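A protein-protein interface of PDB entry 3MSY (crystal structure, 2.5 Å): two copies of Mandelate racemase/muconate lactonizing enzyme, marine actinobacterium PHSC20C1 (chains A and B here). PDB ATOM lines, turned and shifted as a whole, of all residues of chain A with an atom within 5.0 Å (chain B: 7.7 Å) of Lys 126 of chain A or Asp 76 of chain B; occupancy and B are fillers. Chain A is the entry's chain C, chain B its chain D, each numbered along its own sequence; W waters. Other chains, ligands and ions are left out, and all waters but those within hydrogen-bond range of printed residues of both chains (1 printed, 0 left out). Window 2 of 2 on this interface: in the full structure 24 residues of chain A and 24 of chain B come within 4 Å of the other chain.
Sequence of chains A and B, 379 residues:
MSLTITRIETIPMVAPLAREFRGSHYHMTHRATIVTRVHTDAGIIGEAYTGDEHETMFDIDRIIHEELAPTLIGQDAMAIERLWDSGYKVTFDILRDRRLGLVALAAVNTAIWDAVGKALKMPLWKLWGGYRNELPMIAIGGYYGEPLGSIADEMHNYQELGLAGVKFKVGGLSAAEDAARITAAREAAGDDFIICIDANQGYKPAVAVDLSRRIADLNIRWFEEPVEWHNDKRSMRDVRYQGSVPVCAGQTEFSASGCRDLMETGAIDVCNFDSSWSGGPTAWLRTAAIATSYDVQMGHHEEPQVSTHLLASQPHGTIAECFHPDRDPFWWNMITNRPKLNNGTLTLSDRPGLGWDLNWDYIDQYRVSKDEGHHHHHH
No position is printed for both chains.
Of the 8 pairs that touch across the chains among the printed residues, none has its exchanged pair printed and touching as well.
The backbone NH of Gly 130 of chain A is in hydrogen-bond range of the backbone carbonyl oxygen of Trp 125 of chain A (2.8 Å).
The backbone NH of Ile 11 of chain B sits at hydrogen-bond distance from the side-chain carboxylate of Asp 76 of chain B, 3.1 Å away.
The side-chain carboxylate (OD1) of Asp 76 of chain B lies close to the backbone NH (N) of Met 78 of chain B (3.2 Å).
Of chain B, only Asp 76 (2.7 Å) and Met 78 (3.4 Å) come within 4 Å of Lys 126 of chain A.
Of chain A, only Lys 126 comes within 4 Å of Asp 76 of chain B.
Printed residues of chain B within 4 Å of Met 122 of chain A: Met 78.
Printed residues of chain B within 4 Å of Gly 130 of chain A: Ala 79 and Arg 82.
Printed residues of chain A within 4 Å of Met 78 of chain B: Met 122 (3.3 Å) and Lys 126 (3.4 Å).
Of the printed residues of chain A, Ala 79 of chain B touches Gly 129 and Gly 130.
Of the printed residues of chain B, Gly 129 of chain A touches Ala 79 (3.8 Å), Ile 80 (3.6 Å) and Glu 81 (3.1 Å).
Ile 73 of chain B touches none of the printed residues of chain A.
The nearest residue of chain B that does not touch Lys 126 of chain A is Ala 79 of chain B (4.9 Å).
The nearest printed residue of chain A that does not touch Glu 81 of chain B is Trp 128 of chain A (4.5 Å).
Of the 9 printed residues of chain A, 4 touch a printed residue of chain B.
Hydrophobic or aromatic side chains of chain A within 4 Å of the printed part of chain B: Met 122.
Printed residues of chain B that touch a printed residue of chain A: Asp 76, Met 78, Ala 79, Ile 80, Glu 81 and Arg 82.
Hydrophobic or aromatic side chains of chain B within 4 Å of the printed part of chain A: Met 78 and Ala 79.
NZ of Lys 126 of chain A is in salt-bridge range of OD2 of Asp 76 of chain B (2.7 Å).
O of Gly 129 of chain A is in hydrogen-bond range of N of Glu 81 of chain B (3.1 Å).
The backbone carbonyl oxygen (O) of Gly 130 of chain A is in hydrogen-bond range of the guanidinium group (NH1) of Arg 82 of chain B (3.5 Å).
Met 78 of chain B touches Met 122 of chain A.
Lys 126 of chain A touches Met 78 of chain B.
Gly 129 of chain A touches Ala 79 of chain B.
Gly 129 of chain A touches Ile 80 of chain B.
Gly 130 of chain A touches Ala 79 of chain B.
Water W1 bridges the side-chain carboxylate (OE2) of Glu 81 of chain B and the backbone carbonyl oxygen (O) of Trp 128 of chain A.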
ATOM      1  N   MET A 122       1.447 -26.711  34.233  1.00  0.00           N
ATOM      2  CA  MET A 122       1.752 -26.009  32.999  1.00  0.00           C
ATOM      3  C   MET A 122       1.165 -26.695  31.765  1.00  0.00           C
ATOM      4  O   MET A 122       1.358 -27.897  31.561  1.00  0.00           O
ATOM      5  CB  MET A 122       3.268 -25.920  32.827  1.00  0.00           C
ATOM      6  CG  MET A 122       3.946 -25.017  33.811  1.00  0.00           C
ATOM      7  SD  MET A 122       3.620 -23.192  33.297  1.00  0.00           S
ATOM      8  CE  MET A 122       4.864 -23.105  31.795  1.00  0.00           C
ATOM      9  N   PRO A 123       0.425 -25.938  30.935  1.00  0.00           N
ATOM     10  CA  PRO A 123      -0.163 -26.504  29.715  1.00  0.00           C
ATOM     11  C   PRO A 123       1.007 -26.712  28.750  1.00  0.00           C
ATOM     12  O   PRO A 123       1.805 -25.803  28.538  1.00  0.00           O
ATOM     13  CB  PRO A 123      -1.105 -25.403  29.250  1.00  0.00           C
ATOM     14  CG  PRO A 123      -0.380 -24.148  29.676  1.00  0.00           C
ATOM     15  CD  PRO A 123       0.059 -24.515  31.085  1.00  0.00           C
ATOM     16  N   LEU A 124       1.119 -27.902  28.179  1.00  0.00           N
ATOM     17  CA  LEU A 124       2.217 -28.193  27.277  1.00  0.00           C
ATOM     18  C   LEU A 124       2.512 -27.143  26.201  1.00  0.00           C
ATOM     19  O   LEU A 124       3.674 -26.853  25.924  1.00  0.00           O
ATOM     20  CB  LEU A 124       2.023 -29.573  26.635  1.00  0.00           C
ATOM     21  CG  LEU A 124       2.729 -30.780  27.294  1.00  0.00           C
ATOM     22  CD1 LEU A 124       3.834 -30.320  28.239  1.00  0.00           C
ATOM     23  CD2 LEU A 124       1.747 -31.612  28.057  1.00  0.00           C
ATOM     24  N   TRP A 125       1.483 -26.553  25.603  1.00  0.00           N
ATOM     25  CA  TRP A 125       1.724 -25.551  24.567  1.00  0.00           C
ATOM     26  C   TRP A 125       2.613 -24.425  25.084  1.00  0.00           C
ATOM     27  O   TRP A 125       3.282 -23.736  24.305  1.00  0.00           O
ATOM     28  CB  TRP A 125       0.407 -24.964  24.045  1.00  0.00           C
ATOM     29  CG  TRP A 125      -0.332 -24.095  25.032  1.00  0.00           C
ATOM     30  CD1 TRP A 125      -1.389 -24.457  25.813  1.00  0.00           C
ATOM     31  CD2 TRP A 125      -0.062 -22.718  25.331  1.00  0.00           C
ATOM     32  NE1 TRP A 125      -1.798 -23.390  26.578  1.00  0.00           N
ATOM     33  CE2 TRP A 125      -0.999 -22.311  26.302  1.00  0.00           C
ATOM     34  CE3 TRP A 125       0.880 -21.791  24.869  1.00  0.00           C
ATOM     35  CZ2 TRP A 125      -1.024 -21.012  26.823  1.00  0.00           C
ATOM     36  CZ3 TRP A 125       0.856 -20.502  25.384  1.00  0.00           C
ATOM     37  CH2 TRP A 125      -0.091 -20.126  26.353  1.00  0.00           C
ATOM     38  N   LYS A 126       2.625 -24.233  26.398  1.00  0.00           N
ATOM     39  CA  LYS A 126       3.446 -23.180  26.971  1.00  0.00           C
ATOM     40  C   LYS A 126       4.750 -23.728  27.521  1.00  0.00           C
ATOM     41  O   LYS A 126       5.810 -23.132  27.313  1.00  0.00           O
ATOM     42  CB  LYS A 126       2.692 -22.437  28.075  1.00  0.00           C
ATOM     43  CG  LYS A 126       3.492 -21.305  28.688  1.00  0.00           C
ATOM     44  CD  LYS A 126       2.780 -20.637  29.863  1.00  0.00           C
ATOM     45  CE  LYS A 126       1.676 -19.709  29.408  1.00  0.00           C
ATOM     46  NZ  LYS A 126       1.414 -18.649  30.417  1.00  0.00           N
ATOM     47  N   LEU A 127       4.683 -24.860  28.219  1.00  0.00           N
ATOM     48  CA  LEU A 127       5.894 -25.444  28.789  1.00  0.00           C
ATOM     49  C   LEU A 127       6.880 -25.825  27.683  1.00  0.00           C
ATOM     50  O   LEU A 127       8.065 -25.973  27.935  1.00  0.00           O
ATOM     51  CB  LEU A 127       5.560 -26.674  29.639  1.00  0.00           C
ATOM     52  CG  LEU A 127       6.761 -27.306  30.369  1.00  0.00           C
ATOM     53  CD1 LEU A 127       7.201 -26.413  31.525  1.00  0.00           C
ATOM     54  CD2 LEU A 127       6.383 -28.700  30.891  1.00  0.00           C
ATOM     55  N   TRP A 128       6.384 -25.977  26.458  1.00  0.00           N
ATOM     56  CA  TRP A 128       7.246 -26.321  25.335  1.00  0.00           C
ATOM     57  C   TRP A 128       7.705 -25.099  24.561  1.00  0.00           C
ATOM     58  O   TRP A 128       8.499 -25.227  23.637  1.00  0.00           O
ATOM     59  CB  TRP A 128       6.554 -27.285  24.368  1.00  0.00           C
ATOM     60  CG  TRP A 128       6.479 -28.700  24.848  1.00  0.00           C
ATOM     61  CD1 TRP A 128       7.349 -29.332  25.688  1.00  0.00           C
ATOM     62  CD2 TRP A 128       5.502 -29.679  24.473  1.00  0.00           C
ATOM     63  NE1 TRP A 128       6.977 -30.645  25.862  1.00  0.00           N
ATOM     64  CE2 TRP A 128       5.847 -30.885  25.127  1.00  0.00           C
ATOM     65  CE3 TRP A 128       4.367 -29.655  23.648  1.00  0.00           C
ATOM     66  CZ2 TRP A 128       5.099 -32.054  24.981  1.00  0.00           C
ATOM     67  CZ3 TRP A 128       3.621 -30.818  23.501  1.00  0.00           C
ATOM     68  CH2 TRP A 128       3.993 -32.003  24.166  1.00  0.00           C
ATOM     69  N   GLY A 129       7.211 -23.920  24.924  1.00  0.00           N
ATOM     70  CA  GLY A 129       7.616 -22.720  24.219  1.00  0.00           C
ATOM     71  C   GLY A 129       6.678 -21.551  24.442  1.00  0.00           C
ATOM     72  O   GLY A 129       7.111 -20.430  24.714  1.00  0.00           O
ATOM     73  N   GLY A 130       5.383 -21.813  24.313  1.00  0.00           N
ATOM     74  CA  GLY A 130       4.389 -20.777  24.529  1.00  0.00           C
ATOM     75  C   GLY A 130       4.401 -19.646  23.525  1.00  0.00           C
ATOM     76  O   GLY A 130       4.088 -18.508  23.875  1.00  0.00           O
ATOM     77  N   ILE B  11       3.369 -15.404  34.728  1.00  0.00           N
ATOM     78  CA  ILE B  11       3.912 -14.358  35.631  1.00  0.00           C
ATOM     79  C   ILE B  11       4.496 -13.169  34.868  1.00  0.00           C
ATOM     80  O   ILE B  11       5.513 -13.294  34.189  1.00  0.00           O
ATOM     81  CB  ILE B  11       5.000 -14.940  36.574  1.00  0.00           C
ATOM     82  CG1 ILE B  11       6.167 -15.520  35.766  1.00  0.00           C
ATOM     83  CG2 ILE B  11       4.380 -16.030  37.462  1.00  0.00           C
ATOM     84  CD1 ILE B  11       7.392 -15.848  36.612  1.00  0.00           C
ATOM     85  N   PRO B  12       3.830 -12.003  34.955  1.00  0.00           N
ATOM     86  CA  PRO B  12       4.235 -10.753  34.299  1.00  0.00           C
ATOM     87  C   PRO B  12       5.535 -10.154  34.817  1.00  0.00           C
ATOM     88  O   PRO B  12       5.901 -10.332  35.980  1.00  0.00           O
ATOM     89  CB  PRO B  12       3.045  -9.821  34.557  1.00  0.00           C
ATOM     90  CG  PRO B  12       1.894 -10.754  34.509  1.00  0.00           C
ATOM     91  CD  PRO B  12       2.409 -11.927  35.347  1.00  0.00           C
ATOM     92  N   MET B  13       6.216  -9.431  33.936  1.00  0.00           N
ATOM     93  CA  MET B  13       7.464  -8.779  34.282  1.00  0.00           C
ATOM     94  C   MET B  13       7.255  -7.297  34.511  1.00  0.00           C
ATOM     95  O   MET B  13       6.628  -6.611  33.703  1.00  0.00           O
ATOM     96  CB  MET B  13       8.473  -9.010  33.185  1.00  0.00           C
ATOM     97  CG  MET B  13       8.743 -10.459  33.074  1.00  0.00           C
ATOM     98  SD  MET B  13       9.424 -10.892  31.336  1.00  0.00           S
ATOM     99  CE  MET B  13       7.737 -11.282  30.408  1.00  0.00           C
ATOM    100  N   THR B  71       9.945  -4.691  25.157  1.00  0.00           N
ATOM    101  CA  THR B  71       9.295  -5.925  24.718  1.00  0.00           C
ATOM    102  C   THR B  71       9.264  -6.986  25.822  1.00  0.00           C
ATOM    103  O   THR B  71       9.278  -8.190  25.532  1.00  0.00           O
ATOM    104  CB  THR B  71      10.026  -6.535  23.481  1.00  0.00           C
ATOM    105  OG1 THR B  71      11.217  -7.220  23.902  1.00  0.00           O
ATOM    106  CG2 THR B  71      10.408  -5.437  22.488  1.00  0.00           C
ATOM    107  N   LEU B  72       9.213  -6.547  27.080  1.00  0.00           N
ATOM    108  CA  LEU B  72       9.199  -7.479  28.209  1.00  0.00           C
ATOM    109  C   LEU B  72       8.282  -7.040  29.328  1.00  0.00           C
ATOM    110  O   LEU B  72       7.607  -7.856  29.957  1.00  0.00           O
ATOM    111  CB  LEU B  72      10.608  -7.642  28.773  1.00  0.00           C
ATOM    112  CG  LEU B  72      11.647  -8.219  27.816  1.00  0.00           C
ATOM    113  CD1 LEU B  72      12.997  -8.231  28.511  1.00  0.00           C
ATOM    114  CD2 LEU B  72      11.231  -9.627  27.376  1.00  0.00           C
ATOM    115  N   ILE B  73       8.275  -5.742  29.589  1.00  0.00           N
ATOM    116  CA  ILE B  73       7.440  -5.182  30.636  1.00  0.00           C
ATOM    117  C   ILE B  73       5.973  -5.515  30.405  1.00  0.00           C
ATOM    118  O   ILE B  73       5.452  -5.388  29.298  1.00  0.00           O
ATOM    119  CB  ILE B  73       7.625  -3.663  30.717  1.00  0.00           C
ATOM    120  CG1 ILE B  73       9.084  -3.357  31.047  1.00  0.00           C
ATOM    121  CG2 ILE B  73       6.722  -3.077  31.786  1.00  0.00           C
ATOM    122  CD1 ILE B  73       9.564  -4.020  32.331  1.00  0.00           C
ATOM    123  N   GLY B  74       5.315  -5.962  31.464  1.00  0.00           N
ATOM    124  CA  GLY B  74       3.915  -6.307  31.362  1.00  0.00           C
ATOM    125  C   GLY B  74       3.703  -7.626  30.659  1.00  0.00           C
ATOM    126  O   GLY B  74       2.579  -8.119  30.606  1.00  0.00           O
ATOM    127  N   GLN B  75       4.777  -8.207  30.126  1.00  0.00           N
ATOM    128  CA  GLN B  75       4.688  -9.480  29.416  1.00  0.00           C
ATOM    129  C   GLN B  75       4.705 -10.710  30.312  1.00  0.00           C
ATOM    130  O   GLN B  75       5.023 -10.636  31.499  1.00  0.00           O
ATOM    131  CB  GLN B  75       5.828  -9.598  28.407  1.00  0.00           C
ATOM    132  CG  GLN B  75       5.361  -9.672  26.983  1.00  0.00           C
ATOM    133  CD  GLN B  75       4.647  -8.421  26.577  1.00  0.00           C
ATOM    134  OE1 GLN B  75       5.271  -7.370  26.411  1.00  0.00           O
ATOM    135  NE2 GLN B  75       3.328  -8.509  26.432  1.00  0.00           N
ATOM    136  N   ASP B  76       4.361 -11.847  29.721  1.00  0.00           N
ATOM    137  CA  ASP B  76       4.342 -13.126  30.427  1.00  0.00           C
ATOM    138  C   ASP B  76       5.715 -13.771  30.230  1.00  0.00           C
ATOM    139  O   ASP B  76       6.096 -14.099  29.109  1.00  0.00           O
ATOM    140  CB  ASP B  76       3.224 -14.011  29.846  1.00  0.00           C
ATOM    141  CG  ASP B  76       3.112 -15.365  30.537  1.00  0.00           C
ATOM    142  OD1 ASP B  76       3.610 -15.521  31.672  1.00  0.00           O
ATOM    143  OD2 ASP B  76       2.503 -16.279  29.935  1.00  0.00           O
ATOM    144  N   ALA B  77       6.459 -13.935  31.319  1.00  0.00           N
ATOM    145  CA  ALA B  77       7.807 -14.512  31.266  1.00  0.00           C
ATOM    146  C   ALA B  77       7.781 -15.995  30.964  1.00  0.00           C
ATOM    147  O   ALA B  77       8.794 -16.584  30.578  1.00  0.00           O
ATOM    148  CB  ALA B  77       8.544 -14.267  32.586  1.00  0.00           C
ATOM    149  N   MET B  78       6.611 -16.595  31.142  1.00  0.00           N
ATOM    150  CA  MET B  78       6.431 -18.010  30.887  1.00  0.00           C
ATOM    151  C   MET B  78       6.389 -18.280  29.380  1.00  0.00           C
ATOM    152  O   MET B  78       6.464 -19.427  28.950  1.00  0.00           O
ATOM    153  CB  MET B  78       5.130 -18.483  31.535  1.00  0.00           C
ATOM    154  CG  MET B  78       5.212 -19.864  32.155  1.00  0.00           C
ATOM    155  SD  MET B  78       5.659 -19.790  34.057  1.00  0.00           S
ATOM    156  CE  MET B  78       7.168 -18.562  33.949  1.00  0.00           C
ATOM    157  N   ALA B  79       6.264 -17.227  28.581  1.00  0.00           N
ATOM    158  CA  ALA B  79       6.200 -17.372  27.124  1.00  0.00           C
ATOM    159  C   ALA B  79       7.554 -17.075  26.506  1.00  0.00           C
ATOM    160  O   ALA B  79       7.706 -16.115  25.751  1.00  0.00           O
ATOM    161  CB  ALA B  79       5.136 -16.418  26.545  1.00  0.00           C
ATOM    162  N   ILE B  80       8.538 -17.907  26.802  1.00  0.00           N
ATOM    163  CA  ILE B  80       9.870 -17.659  26.294  1.00  0.00           C
ATOM    164  C   ILE B  80      10.003 -17.555  24.773  1.00  0.00           C
ATOM    165  O   ILE B  80      10.538 -16.566  24.274  1.00  0.00           O
ATOM    166  CB  ILE B  80      10.868 -18.697  26.851  1.00  0.00           C
ATOM    167  CG1 ILE B  80      10.903 -18.586  28.375  1.00  0.00           C
ATOM    168  CG2 ILE B  80      12.270 -18.423  26.313  1.00  0.00           C
ATOM    169  CD1 ILE B  80      11.827 -19.568  29.054  1.00  0.00           C
ATOM    170  N   GLU B  81       9.523 -18.554  24.038  1.00  0.00           N
ATOM    171  CA  GLU B  81       9.636 -18.518  22.589  1.00  0.00           C
ATOM    172  C   GLU B  81       9.121 -17.205  22.022  1.00  0.00           C
ATOM    173  O   GLU B  81       9.756 -16.601  21.169  1.00  0.00           O
ATOM    174  CB  GLU B  81       8.880 -19.693  21.952  1.00  0.00           C
ATOM    175  CG  GLU B  81       9.529 -21.066  22.146  1.00  0.00           C
ATOM    176  CD  GLU B  81      10.997 -21.102  21.739  1.00  0.00           C
ATOM    177  OE1 GLU B  81      11.370 -20.388  20.782  1.00  0.00           O
ATOM    178  OE2 GLU B  81      11.779 -21.857  22.365  1.00  0.00           O
ATOM    179  N   ARG B  82       7.968 -16.765  22.502  1.00  0.00           N
ATOM    180  CA  ARG B  82       7.375 -15.521  22.046  1.00  0.00           C
ATOM    181  C   ARG B  82       8.288 -14.351  22.380  1.00  0.00           C
ATOM    182  O   ARG B  82       8.584 -13.507  21.531  1.00  0.00           O
ATOM    183  CB  ARG B  82       6.006 -15.328  22.708  1.00  0.00           C
ATOM    184  CG  ARG B  82       5.182 -14.181  22.141  1.00  0.00           C
ATOM    185  CD  ARG B  82       3.730 -14.313  22.549  1.00  0.00           C
ATOM    186  NE  ARG B  82       3.515 -13.962  23.948  1.00  0.00           N
ATOM    187  CZ  ARG B  82       2.722 -14.629  24.785  1.00  0.00           C
ATOM    188  NH1 ARG B  82       2.058 -15.706  24.376  1.00  0.00           N
ATOM    189  NH2 ARG B  82       2.585 -14.205  26.036  1.00  0.00           N
ATOM    190  N   LEU B  83       8.740 -14.301  23.626  1.00  0.00           N
ATOM    191  CA  LEU B  83       9.617 -13.222  24.054  1.00  0.00           C
ATOM    192  C   LEU B  83      10.930 -13.212  23.299  1.00  0.00           C
ATOM    193  O   LEU B  83      11.399 -12.154  22.894  1.00  0.00           O
ATOM    194  CB  LEU B  83       9.914 -13.334  25.548  1.00  0.00           C
ATOM    195  CG  LEU B  83       8.740 -13.184  26.510  1.00  0.00           C
ATOM    196  CD1 LEU B  83       9.267 -13.273  27.934  1.00  0.00           C
ATOM    197  CD2 LEU B  83       8.031 -11.853  26.265  1.00  0.00           C
ATOM    198  N   ILE B 112      15.592 -14.479  32.511  1.00  0.00           N
ATOM    199  CA  ILE B 112      14.209 -14.950  32.449  1.00  0.00           C
ATOM    200  C   ILE B 112      14.101 -16.432  32.763  1.00  0.00           C
ATOM    201  O   ILE B 112      13.180 -16.852  33.454  1.00  0.00           O
ATOM    202  CB  ILE B 112      13.579 -14.696  31.063  1.00  0.00           C
ATOM    203  CG1 ILE B 112      13.485 -13.194  30.810  1.00  0.00           C
ATOM    204  CG2 ILE B 112      12.181 -15.299  30.998  1.00  0.00           C
ATOM    205  CD1 ILE B 112      13.002 -12.848  29.413  1.00  0.00           C
ATOM    206  N   VAL B 116      11.676 -18.430  35.466  1.00  0.00           N
ATOM    207  CA  VAL B 116      10.706 -19.493  35.250  1.00  0.00           C
ATOM    208  C   VAL B 116      11.089 -20.744  36.031  1.00  0.00           C
ATOM    209  O   VAL B 116      10.222 -21.494  36.484  1.00  0.00           O
ATOM    210  CB  VAL B 116      10.550 -19.827  33.747  1.00  0.00           C
ATOM    211  CG1 VAL B 116      10.321 -18.540  32.952  1.00  0.00           C
ATOM    212  CG2 VAL B 116      11.767 -20.577  33.248  1.00  0.00           C
HETATM  213  O   HOH W   1      11.181 -24.326  22.426  1.00  0.00           O
